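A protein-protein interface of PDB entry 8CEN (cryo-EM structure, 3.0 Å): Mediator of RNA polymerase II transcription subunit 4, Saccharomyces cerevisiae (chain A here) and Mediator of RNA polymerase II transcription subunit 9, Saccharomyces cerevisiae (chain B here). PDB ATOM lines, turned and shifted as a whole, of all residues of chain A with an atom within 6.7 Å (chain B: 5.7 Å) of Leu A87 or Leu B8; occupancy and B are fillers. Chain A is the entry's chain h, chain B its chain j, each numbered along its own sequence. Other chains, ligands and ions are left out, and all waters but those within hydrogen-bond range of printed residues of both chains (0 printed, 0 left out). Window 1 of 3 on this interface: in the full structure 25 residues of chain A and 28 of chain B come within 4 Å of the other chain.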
ATOM      1  N   LEU A  42      16.232  27.309  32.243  1.00  0.00           N
ATOM      2  CA  LEU A  42      17.485  27.121  32.969  1.00  0.00           C
ATOM      3  C   LEU A  42      18.332  28.390  32.976  1.00  0.00           C
ATOM      4  O   LEU A  42      19.131  28.598  33.904  1.00  0.00           O
ATOM      5  CB  LEU A  42      18.264  25.953  32.355  1.00  0.00           C
ATOM      6  CG  LEU A  42      19.588  25.514  32.990  1.00  0.00           C
ATOM      7  CD1 LEU A  42      19.371  25.068  34.425  1.00  0.00           C
ATOM      8  CD2 LEU A  42      20.241  24.406  32.177  1.00  0.00           C
ATOM      9  N   GLU A  82      17.580  20.049  40.640  1.00  0.00           N
ATOM     10  CA  GLU A  82      16.621  19.274  39.854  1.00  0.00           C
ATOM     11  C   GLU A  82      16.448  19.779  38.420  1.00  0.00           C
ATOM     12  O   GLU A  82      15.966  19.014  37.581  1.00  0.00           O
ATOM     13  CB  GLU A  82      15.266  19.110  40.565  1.00  0.00           C
ATOM     14  CG  GLU A  82      15.265  18.152  41.795  1.00  0.00           C
ATOM     15  CD  GLU A  82      15.725  18.711  43.125  1.00  0.00           C
ATOM     16  OE1 GLU A  82      16.023  19.902  43.224  1.00  0.00           O
ATOM     17  OE2 GLU A  82      15.788  17.930  44.096  1.00  0.00           O
ATOM     18  N   ASN A  83      16.914  20.984  38.073  1.00  0.00           N
ATOM     19  CA  ASN A  83      17.010  21.309  36.654  1.00  0.00           C
ATOM     20  C   ASN A  83      18.138  20.533  35.982  1.00  0.00           C
ATOM     21  O   ASN A  83      18.013  20.155  34.815  1.00  0.00           O
ATOM     22  CB  ASN A  83      17.198  22.813  36.459  1.00  0.00           C
ATOM     23  CG  ASN A  83      15.880  23.549  36.303  1.00  0.00           C
ATOM     24  OD1 ASN A  83      14.824  23.039  36.678  1.00  0.00           O
ATOM     25  ND2 ASN A  83      15.936  24.753  35.747  1.00  0.00           N
ATOM     26  N   VAL A  84      19.230  20.275  36.705  1.00  0.00           N
ATOM     27  CA  VAL A  84      20.284  19.401  36.193  1.00  0.00           C
ATOM     28  C   VAL A  84      19.762  17.975  36.024  1.00  0.00           C
ATOM     29  O   VAL A  84      20.066  17.297  35.031  1.00  0.00           O
ATOM     30  CB  VAL A  84      21.515  19.467  37.121  1.00  0.00           C
ATOM     31  CG1 VAL A  84      22.469  18.306  36.873  1.00  0.00           C
ATOM     32  CG2 VAL A  84      22.240  20.790  36.940  1.00  0.00           C
ATOM     33  N   LYS A  85      18.958  17.506  36.982  1.00  0.00           N
ATOM     34  CA  LYS A  85      18.358  16.174  36.863  1.00  0.00           C
ATOM     35  C   LYS A  85      17.404  16.088  35.670  1.00  0.00           C
ATOM     36  O   LYS A  85      17.422  15.107  34.910  1.00  0.00           O
ATOM     37  CB  LYS A  85      17.637  15.805  38.159  1.00  0.00           C
ATOM     38  CG  LYS A  85      18.449  14.917  39.091  1.00  0.00           C
ATOM     39  CD  LYS A  85      19.508  15.711  39.837  1.00  0.00           C
ATOM     40  CE  LYS A  85      20.454  14.795  40.598  1.00  0.00           C
ATOM     41  NZ  LYS A  85      21.258  15.537  41.610  1.00  0.00           N
ATOM     42  N   LEU A  86      16.575  17.113  35.466  1.00  0.00           N
ATOM     43  CA  LEU A  86      15.711  17.094  34.294  1.00  0.00           C
ATOM     44  C   LEU A  86      16.475  17.371  33.002  1.00  0.00           C
ATOM     45  O   LEU A  86      15.975  17.046  31.927  1.00  0.00           O
ATOM     46  CB  LEU A  86      14.542  18.071  34.454  1.00  0.00           C
ATOM     47  CG  LEU A  86      13.286  17.561  35.191  1.00  0.00           C
ATOM     48  CD1 LEU A  86      12.658  16.407  34.417  1.00  0.00           C
ATOM     49  CD2 LEU A  86      13.500  17.161  36.649  1.00  0.00           C
ATOM     50  N   LEU A  87      17.691  17.920  33.074  1.00  0.00           N
ATOM     51  CA  LEU A  87      18.550  17.971  31.891  1.00  0.00           C
ATOM     52  C   LEU A  87      19.119  16.591  31.568  1.00  0.00           C
ATOM     53  O   LEU A  87      19.303  16.236  30.395  1.00  0.00           O
ATOM     54  CB  LEU A  87      19.667  18.995  32.107  1.00  0.00           C
ATOM     55  CG  LEU A  87      20.713  19.223  31.013  1.00  0.00           C
ATOM     56  CD1 LEU A  87      20.996  20.708  30.868  1.00  0.00           C
ATOM     57  CD2 LEU A  87      22.007  18.478  31.320  1.00  0.00           C
ATOM     58  N   ALA A  88      19.411  15.802  32.604  1.00  0.00           N
ATOM     59  CA  ALA A  88      19.750  14.399  32.384  1.00  0.00           C
ATOM     60  C   ALA A  88      18.581  13.645  31.761  1.00  0.00           C
ATOM     61  O   ALA A  88      18.786  12.726  30.960  1.00  0.00           O
ATOM     62  CB  ALA A  88      20.179  13.743  33.697  1.00  0.00           C
ATOM     63  N   GLU A  89      17.351  14.018  32.124  1.00  0.00           N
ATOM     64  CA  GLU A  89      16.175  13.489  31.431  1.00  0.00           C
ATOM     65  C   GLU A  89      16.074  14.032  30.001  1.00  0.00           C
ATOM     66  O   GLU A  89      15.602  13.331  29.090  1.00  0.00           O
ATOM     67  CB  GLU A  89      14.911  13.817  32.228  1.00  0.00           C
ATOM     68  CG  GLU A  89      13.643  13.148  31.716  1.00  0.00           C
ATOM     69  CD  GLU A  89      12.819  14.057  30.823  1.00  0.00           C
ATOM     70  OE1 GLU A  89      13.011  15.289  30.887  1.00  0.00           O
ATOM     71  OE2 GLU A  89      11.982  13.539  30.055  1.00  0.00           O
ATOM     72  N   TYR A  90      16.488  15.291  29.798  1.00  0.00           N
ATOM     73  CA  TYR A  90      16.510  15.894  28.468  1.00  0.00           C
ATOM     74  C   TYR A  90      17.427  15.146  27.517  1.00  0.00           C
ATOM     75  O   TYR A  90      17.143  15.080  26.319  1.00  0.00           O
ATOM     76  CB  TYR A  90      16.947  17.361  28.534  1.00  0.00           C
ATOM     77  CG  TYR A  90      15.923  18.331  29.070  1.00  0.00           C
ATOM     78  CD1 TYR A  90      14.582  17.985  29.149  1.00  0.00           C
ATOM     79  CD2 TYR A  90      16.299  19.604  29.483  1.00  0.00           C
ATOM     80  CE1 TYR A  90      13.646  18.877  29.627  1.00  0.00           C
ATOM     81  CE2 TYR A  90      15.370  20.503  29.968  1.00  0.00           C
ATOM     82  CZ  TYR A  90      14.044  20.133  30.040  1.00  0.00           C
ATOM     83  OH  TYR A  90      13.113  21.025  30.521  1.00  0.00           O
ATOM     84  N   ASP A  91      18.535  14.605  28.025  1.00  0.00           N
ATOM     85  CA  ASP A  91      19.428  13.811  27.180  1.00  0.00           C
ATOM     86  C   ASP A  91      18.712  12.581  26.619  1.00  0.00           C
ATOM     87  O   ASP A  91      18.810  12.275  25.420  1.00  0.00           O
ATOM     88  CB  ASP A  91      20.670  13.400  27.974  1.00  0.00           C
ATOM     89  CG  ASP A  91      21.890  13.197  27.092  1.00  0.00           C
ATOM     90  OD1 ASP A  91      21.744  12.657  25.975  1.00  0.00           O
ATOM     91  OD2 ASP A  91      23.000  13.581  27.518  1.00  0.00           O
ATOM     92  N   ASN A  92      17.956  11.881  27.471  1.00  0.00           N
ATOM     93  CA  ASN A  92      17.237  10.689  27.029  1.00  0.00           C
ATOM     94  C   ASN A  92      16.093  11.039  26.083  1.00  0.00           C
ATOM     95  O   ASN A  92      15.853  10.326  25.095  1.00  0.00           O
ATOM     96  CB  ASN A  92      16.716   9.914  28.239  1.00  0.00           C
ATOM     97  CG  ASN A  92      17.796   9.652  29.270  1.00  0.00           C
ATOM     98  OD1 ASN A  92      17.613   9.914  30.459  1.00  0.00           O
ATOM     99  ND2 ASN A  92      18.931   9.130  28.817  1.00  0.00           N
ATOM    100  N   TYR A  94      16.049  13.600  24.164  1.00  0.00           N
ATOM    101  CA  TYR A  94      16.708  13.996  22.925  1.00  0.00           C
ATOM    102  C   TYR A  94      17.104  12.788  22.091  1.00  0.00           C
ATOM    103  O   TYR A  94      16.905  12.788  20.872  1.00  0.00           O
ATOM    104  CB  TYR A  94      17.934  14.858  23.223  1.00  0.00           C
ATOM    105  CG  TYR A  94      18.728  15.224  21.986  1.00  0.00           C
ATOM    106  CD1 TYR A  94      18.254  16.169  21.084  1.00  0.00           C
ATOM    107  CD2 TYR A  94      19.958  14.629  21.723  1.00  0.00           C
ATOM    108  CE1 TYR A  94      18.978  16.508  19.955  1.00  0.00           C
ATOM    109  CE2 TYR A  94      20.687  14.960  20.596  1.00  0.00           C
ATOM    110  CZ  TYR A  94      20.192  15.900  19.717  1.00  0.00           C
ATOM    111  OH  TYR A  94      20.915  16.234  18.595  1.00  0.00           O
ATOM    112  N   ASN B   5      24.539  13.010  24.790  1.00  0.00           N
ATOM    113  CA  ASN B   5      24.945  13.987  23.791  1.00  0.00           C
ATOM    114  C   ASN B   5      26.193  14.730  24.267  1.00  0.00           C
ATOM    115  O   ASN B   5      26.427  14.882  25.469  1.00  0.00           O
ATOM    116  CB  ASN B   5      23.798  14.961  23.514  1.00  0.00           C
ATOM    117  CG  ASN B   5      24.122  15.953  22.417  1.00  0.00           C
ATOM    118  OD1 ASN B   5      24.474  17.099  22.685  1.00  0.00           O
ATOM    119  ND2 ASN B   5      24.002  15.515  21.169  1.00  0.00           N
ATOM    120  N   ASN B   6      27.001  15.183  23.303  1.00  0.00           N
ATOM    121  CA  ASN B   6      28.342  15.681  23.607  1.00  0.00           C
ATOM    122  C   ASN B   6      28.307  16.974  24.418  1.00  0.00           C
ATOM    123  O   ASN B   6      28.916  17.057  25.492  1.00  0.00           O
ATOM    124  CB  ASN B   6      29.132  15.872  22.308  1.00  0.00           C
ATOM    125  CG  ASN B   6      28.329  16.575  21.229  1.00  0.00           C
ATOM    126  OD1 ASN B   6      27.191  16.985  21.453  1.00  0.00           O
ATOM    127  ND2 ASN B   6      28.924  16.722  20.050  1.00  0.00           N
ATOM    128  N   VAL B   7      27.593  17.993  23.928  1.00  0.00           N
ATOM    129  CA  VAL B   7      27.589  19.284  24.615  1.00  0.00           C
ATOM    130  C   VAL B   7      26.834  19.190  25.934  1.00  0.00           C
ATOM    131  O   VAL B   7      27.177  19.881  26.902  1.00  0.00           O
ATOM    132  CB  VAL B   7      27.032  20.399  23.705  1.00  0.00           C
ATOM    133  CG1 VAL B   7      27.951  20.613  22.512  1.00  0.00           C
ATOM    134  CG2 VAL B   7      25.617  20.093  23.239  1.00  0.00           C
ATOM    135  N   LEU B   8      25.820  18.320  26.005  1.00  0.00           N
ATOM    136  CA  LEU B   8      25.151  18.054  27.273  1.00  0.00           C
ATOM    137  C   LEU B   8      26.114  17.427  28.271  1.00  0.00           C
ATOM    138  O   LEU B   8      26.101  17.772  29.458  1.00  0.00           O
ATOM    139  CB  LEU B   8      23.934  17.149  27.062  1.00  0.00           C
ATOM    140  CG  LEU B   8      22.596  17.739  26.586  1.00  0.00           C
ATOM    141  CD1 LEU B   8      22.082  18.775  27.576  1.00  0.00           C
ATOM    142  CD2 LEU B   8      22.638  18.307  25.172  1.00  0.00           C
ATOM    143  N   ASN B   9      26.972  16.516  27.802  1.00  0.00           N
ATOM    144  CA  ASN B   9      27.979  15.921  28.675  1.00  0.00           C
ATOM    145  C   ASN B   9      28.988  16.959  29.158  1.00  0.00           C
ATOM    146  O   ASN B   9      29.345  16.972  30.343  1.00  0.00           O
ATOM    147  CB  ASN B   9      28.690  14.778  27.954  1.00  0.00           C
ATOM    148  CG  ASN B   9      27.879  13.497  27.954  1.00  0.00           C
ATOM    149  OD1 ASN B   9      27.782  12.808  26.938  1.00  0.00           O
ATOM    150  ND2 ASN B   9      27.289  13.170  29.099  1.00  0.00           N
ATOM    151  N   GLN B  10      29.456  17.838  28.261  1.00  0.00           N
ATOM    152  CA  GLN B  10      30.417  18.854  28.691  1.00  0.00           C
ATOM    153  C   GLN B  10      29.802  19.825  29.695  1.00  0.00           C
ATOM    154  O   GLN B  10      30.439  20.152  30.703  1.00  0.00           O
ATOM    155  CB  GLN B  10      31.031  19.631  27.518  1.00  0.00           C
ATOM    156  CG  GLN B  10      32.139  18.897  26.755  1.00  0.00           C
ATOM    157  CD  GLN B  10      31.719  18.362  25.406  1.00  0.00           C
ATOM    158  OE1 GLN B  10      30.832  18.914  24.760  1.00  0.00           O
ATOM    159  NE2 GLN B  10      32.355  17.281  24.971  1.00  0.00           N
ATOM    160  N   ILE B  11      28.562  20.274  29.463  1.00  0.00           N
ATOM    161  CA  ILE B  11      27.963  21.198  30.427  1.00  0.00           C
ATOM    162  C   ILE B  11      27.653  20.488  31.745  1.00  0.00           C
ATOM    163  O   ILE B  11      27.814  21.079  32.821  1.00  0.00           O
ATOM    164  CB  ILE B  11      26.723  21.917  29.850  1.00  0.00           C
ATOM    165  CG1 ILE B  11      25.588  20.949  29.514  1.00  0.00           C
ATOM    166  CG2 ILE B  11      27.106  22.738  28.625  1.00  0.00           C
ATOM    167  CD1 ILE B  11      24.339  21.627  28.992  1.00  0.00           C
ATOM    168  N   HIS B  12      27.264  19.206  31.695  1.00  0.00           N
ATOM    169  CA  HIS B  12      26.966  18.466  32.917  1.00  0.00           C
ATOM    170  C   HIS B  12      28.215  18.245  33.761  1.00  0.00           C
ATOM    171  O   HIS B  12      28.179  18.425  34.983  1.00  0.00           O
ATOM    172  CB  HIS B  12      26.307  17.130  32.573  1.00  0.00           C
ATOM    173  CG  HIS B  12      25.929  16.316  33.773  1.00  0.00           C
ATOM    174  ND1 HIS B  12      26.692  15.262  34.227  1.00  0.00           N
ATOM    175  CD2 HIS B  12      24.869  16.401  34.610  1.00  0.00           C
ATOM    176  CE1 HIS B  12      26.119  14.734  35.294  1.00  0.00           C
ATOM    177  NE2 HIS B  12      25.010  15.407  35.547  1.00  0.00           N
ATOM    178  N   GLN B  13      29.331  17.873  33.137  1.00  0.00           N
ATOM    179  CA  GLN B  13      30.560  17.653  33.891  1.00  0.00           C
ATOM    180  C   GLN B  13      31.420  18.904  34.048  1.00  0.00           C
ATOM    181  O   GLN B  13      32.513  18.808  34.616  1.00  0.00           O
ATOM    182  CB  GLN B  13      31.391  16.520  33.273  1.00  0.00           C
ATOM    183  CG  GLN B  13      31.002  15.126  33.777  1.00  0.00           C
ATOM    184  CD  GLN B  13      30.047  14.379  32.868  1.00  0.00           C
ATOM    185  OE1 GLN B  13      30.007  14.608  31.663  1.00  0.00           O
ATOM    186  NE2 GLN B  13      29.268  13.473  33.450  1.00  0.00           N
ATOM    187  N   ASN B 108      25.439  26.352  21.236  1.00  0.00           N
ATOM    188  CA  ASN B 108      24.714  25.214  20.687  1.00  0.00           C
ATOM    189  C   ASN B 108      23.232  25.556  20.593  1.00  0.00           C
ATOM    190  O   ASN B 108      22.657  26.107  21.537  1.00  0.00           O
ATOM    191  CB  ASN B 108      24.942  23.967  21.546  1.00  0.00           C
ATOM    192  CG  ASN B 108      24.484  22.698  20.864  1.00  0.00           C
ATOM    193  OD1 ASN B 108      23.526  22.064  21.293  1.00  0.00           O
ATOM    194  ND2 ASN B 108      25.169  22.323  19.790  1.00  0.00           N
ATOM    195  N   THR B 111      20.089  22.265  21.543  1.00  0.00           N
ATOM    196  CA  THR B 111      19.928  22.202  22.993  1.00  0.00           C
ATOM    197  C   THR B 111      19.250  23.463  23.524  1.00  0.00           C
ATOM    198  O   THR B 111      18.458  23.395  24.475  1.00  0.00           O
ATOM    199  CB  THR B 111      21.292  21.994  23.657  1.00  0.00           C
ATOM    200  OG1 THR B 111      21.898  20.808  23.127  1.00  0.00           O
ATOM    201  CG2 THR B 111      21.159  21.831  25.167  1.00  0.00           C
ATOM    202  N   LEU B 114      15.767  22.840  22.961  1.00  0.00           N
ATOM    203  CA  LEU B 114      15.293  21.836  23.914  1.00  0.00           C
ATOM    204  C   LEU B 114      14.983  22.451  25.273  1.00  0.00           C
ATOM    205  O   LEU B 114      14.013  22.058  25.932  1.00  0.00           O
ATOM    206  CB  LEU B 114      16.330  20.728  24.076  1.00  0.00           C
ATOM    207  CG  LEU B 114      16.477  19.671  22.987  1.00  0.00           C
ATOM    208  CD1 LEU B 114      17.267  18.511  23.551  1.00  0.00           C
ATOM    209  CD2 LEU B 114      15.122  19.208  22.476  1.00  0.00           C
ATOM    210  N   LEU B 115      15.801  23.407  25.711  1.00  0.00           N
ATOM    211  CA  LEU B 115      15.654  23.984  27.043  1.00  0.00           C
ATOM    212  C   LEU B 115      14.450  24.912  27.175  1.00  0.00           C
ATOM    213  O   LEU B 115      14.173  25.376  28.285  1.00  0.00           O
ATOM    214  CB  LEU B 115      16.929  24.741  27.427  1.00  0.00           C
ATOM    215  CG  LEU B 115      17.947  24.033  28.328  1.00  0.00           C
ATOM    216  CD1 LEU B 115      18.417  22.716  27.728  1.00  0.00           C
ATOM    217  CD2 LEU B 115      19.132  24.947  28.602  1.00  0.00           C
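Of chain A, only Leu A87 (3.7 Å) and Asp A91 (3.7 Å) come within 4 Å of Leu B8. Printed residues of chain B within 4 Å of Val A84: His B12 (3.8 Å). Printed residues of chain A within 4 Å of Ile B11: Leu A87. Of the printed residues of chain A, His B12 touches Val A84. Gln B13 touches none of the printed residues of chain A. Leu A86 touches none of the printed residues of chain B. The nearest residue of chain A that does not touch Leu B8 is Tyr A90 (5.4 Å).
Of the 13 printed residues of chain A, 5 touch a printed residue of chain B. Hydrophobic or aromatic side chains of chain A that line the printed part of chain B: Leu A42, Val A84, Leu A87 and Tyr A94. Hydrophobic or aromatic side chains of chain B that line the printed part of chain A: Leu B8, Ile B11, His B12, Leu B114 and Leu B115. Among the printed residues, 8 pairs touch across the chains. Among the printed residues, no Asp or Glu carboxylate lies within 4 Å of a Lys or Arg side-chain nitrogen of the other chain.
The side-chain carboxylate (OD1) of Asp A91 sits at hydrogen-bond distance from the backbone NH (N) of Asn B5 (3.1 Å).
O of Asn B5 sits close to OD1 of Asn B9 (2.9 Å). The side-chain amide oxygen of Asn B6 lies close to the side-chain amide oxygen of Asn B5, at 3.0 Å. A ring nitrogen (ND1) of His B12 lies within hydrogen-bond range of the side-chain amide nitrogen of Gln B13 (3.2 Å). N of Val B7 sits close to OD1 of Asn B5 (3.5 Å).
Leu B115 touches Leu A42 (CD2 to CD2, 3.8 Å). CD2 of His B12 touches CG1 of Val A84 (3.8 Å). Leu B8 touches Leu A87. Ile B11 touches Leu A87. OD2 of Asp A91 touches CB of Leu B8, 3.7 Å away. Tyr A94 touches Asn B5. Tyr A94 touches Leu B114 (CD1 to CD1, 3.5 Å).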
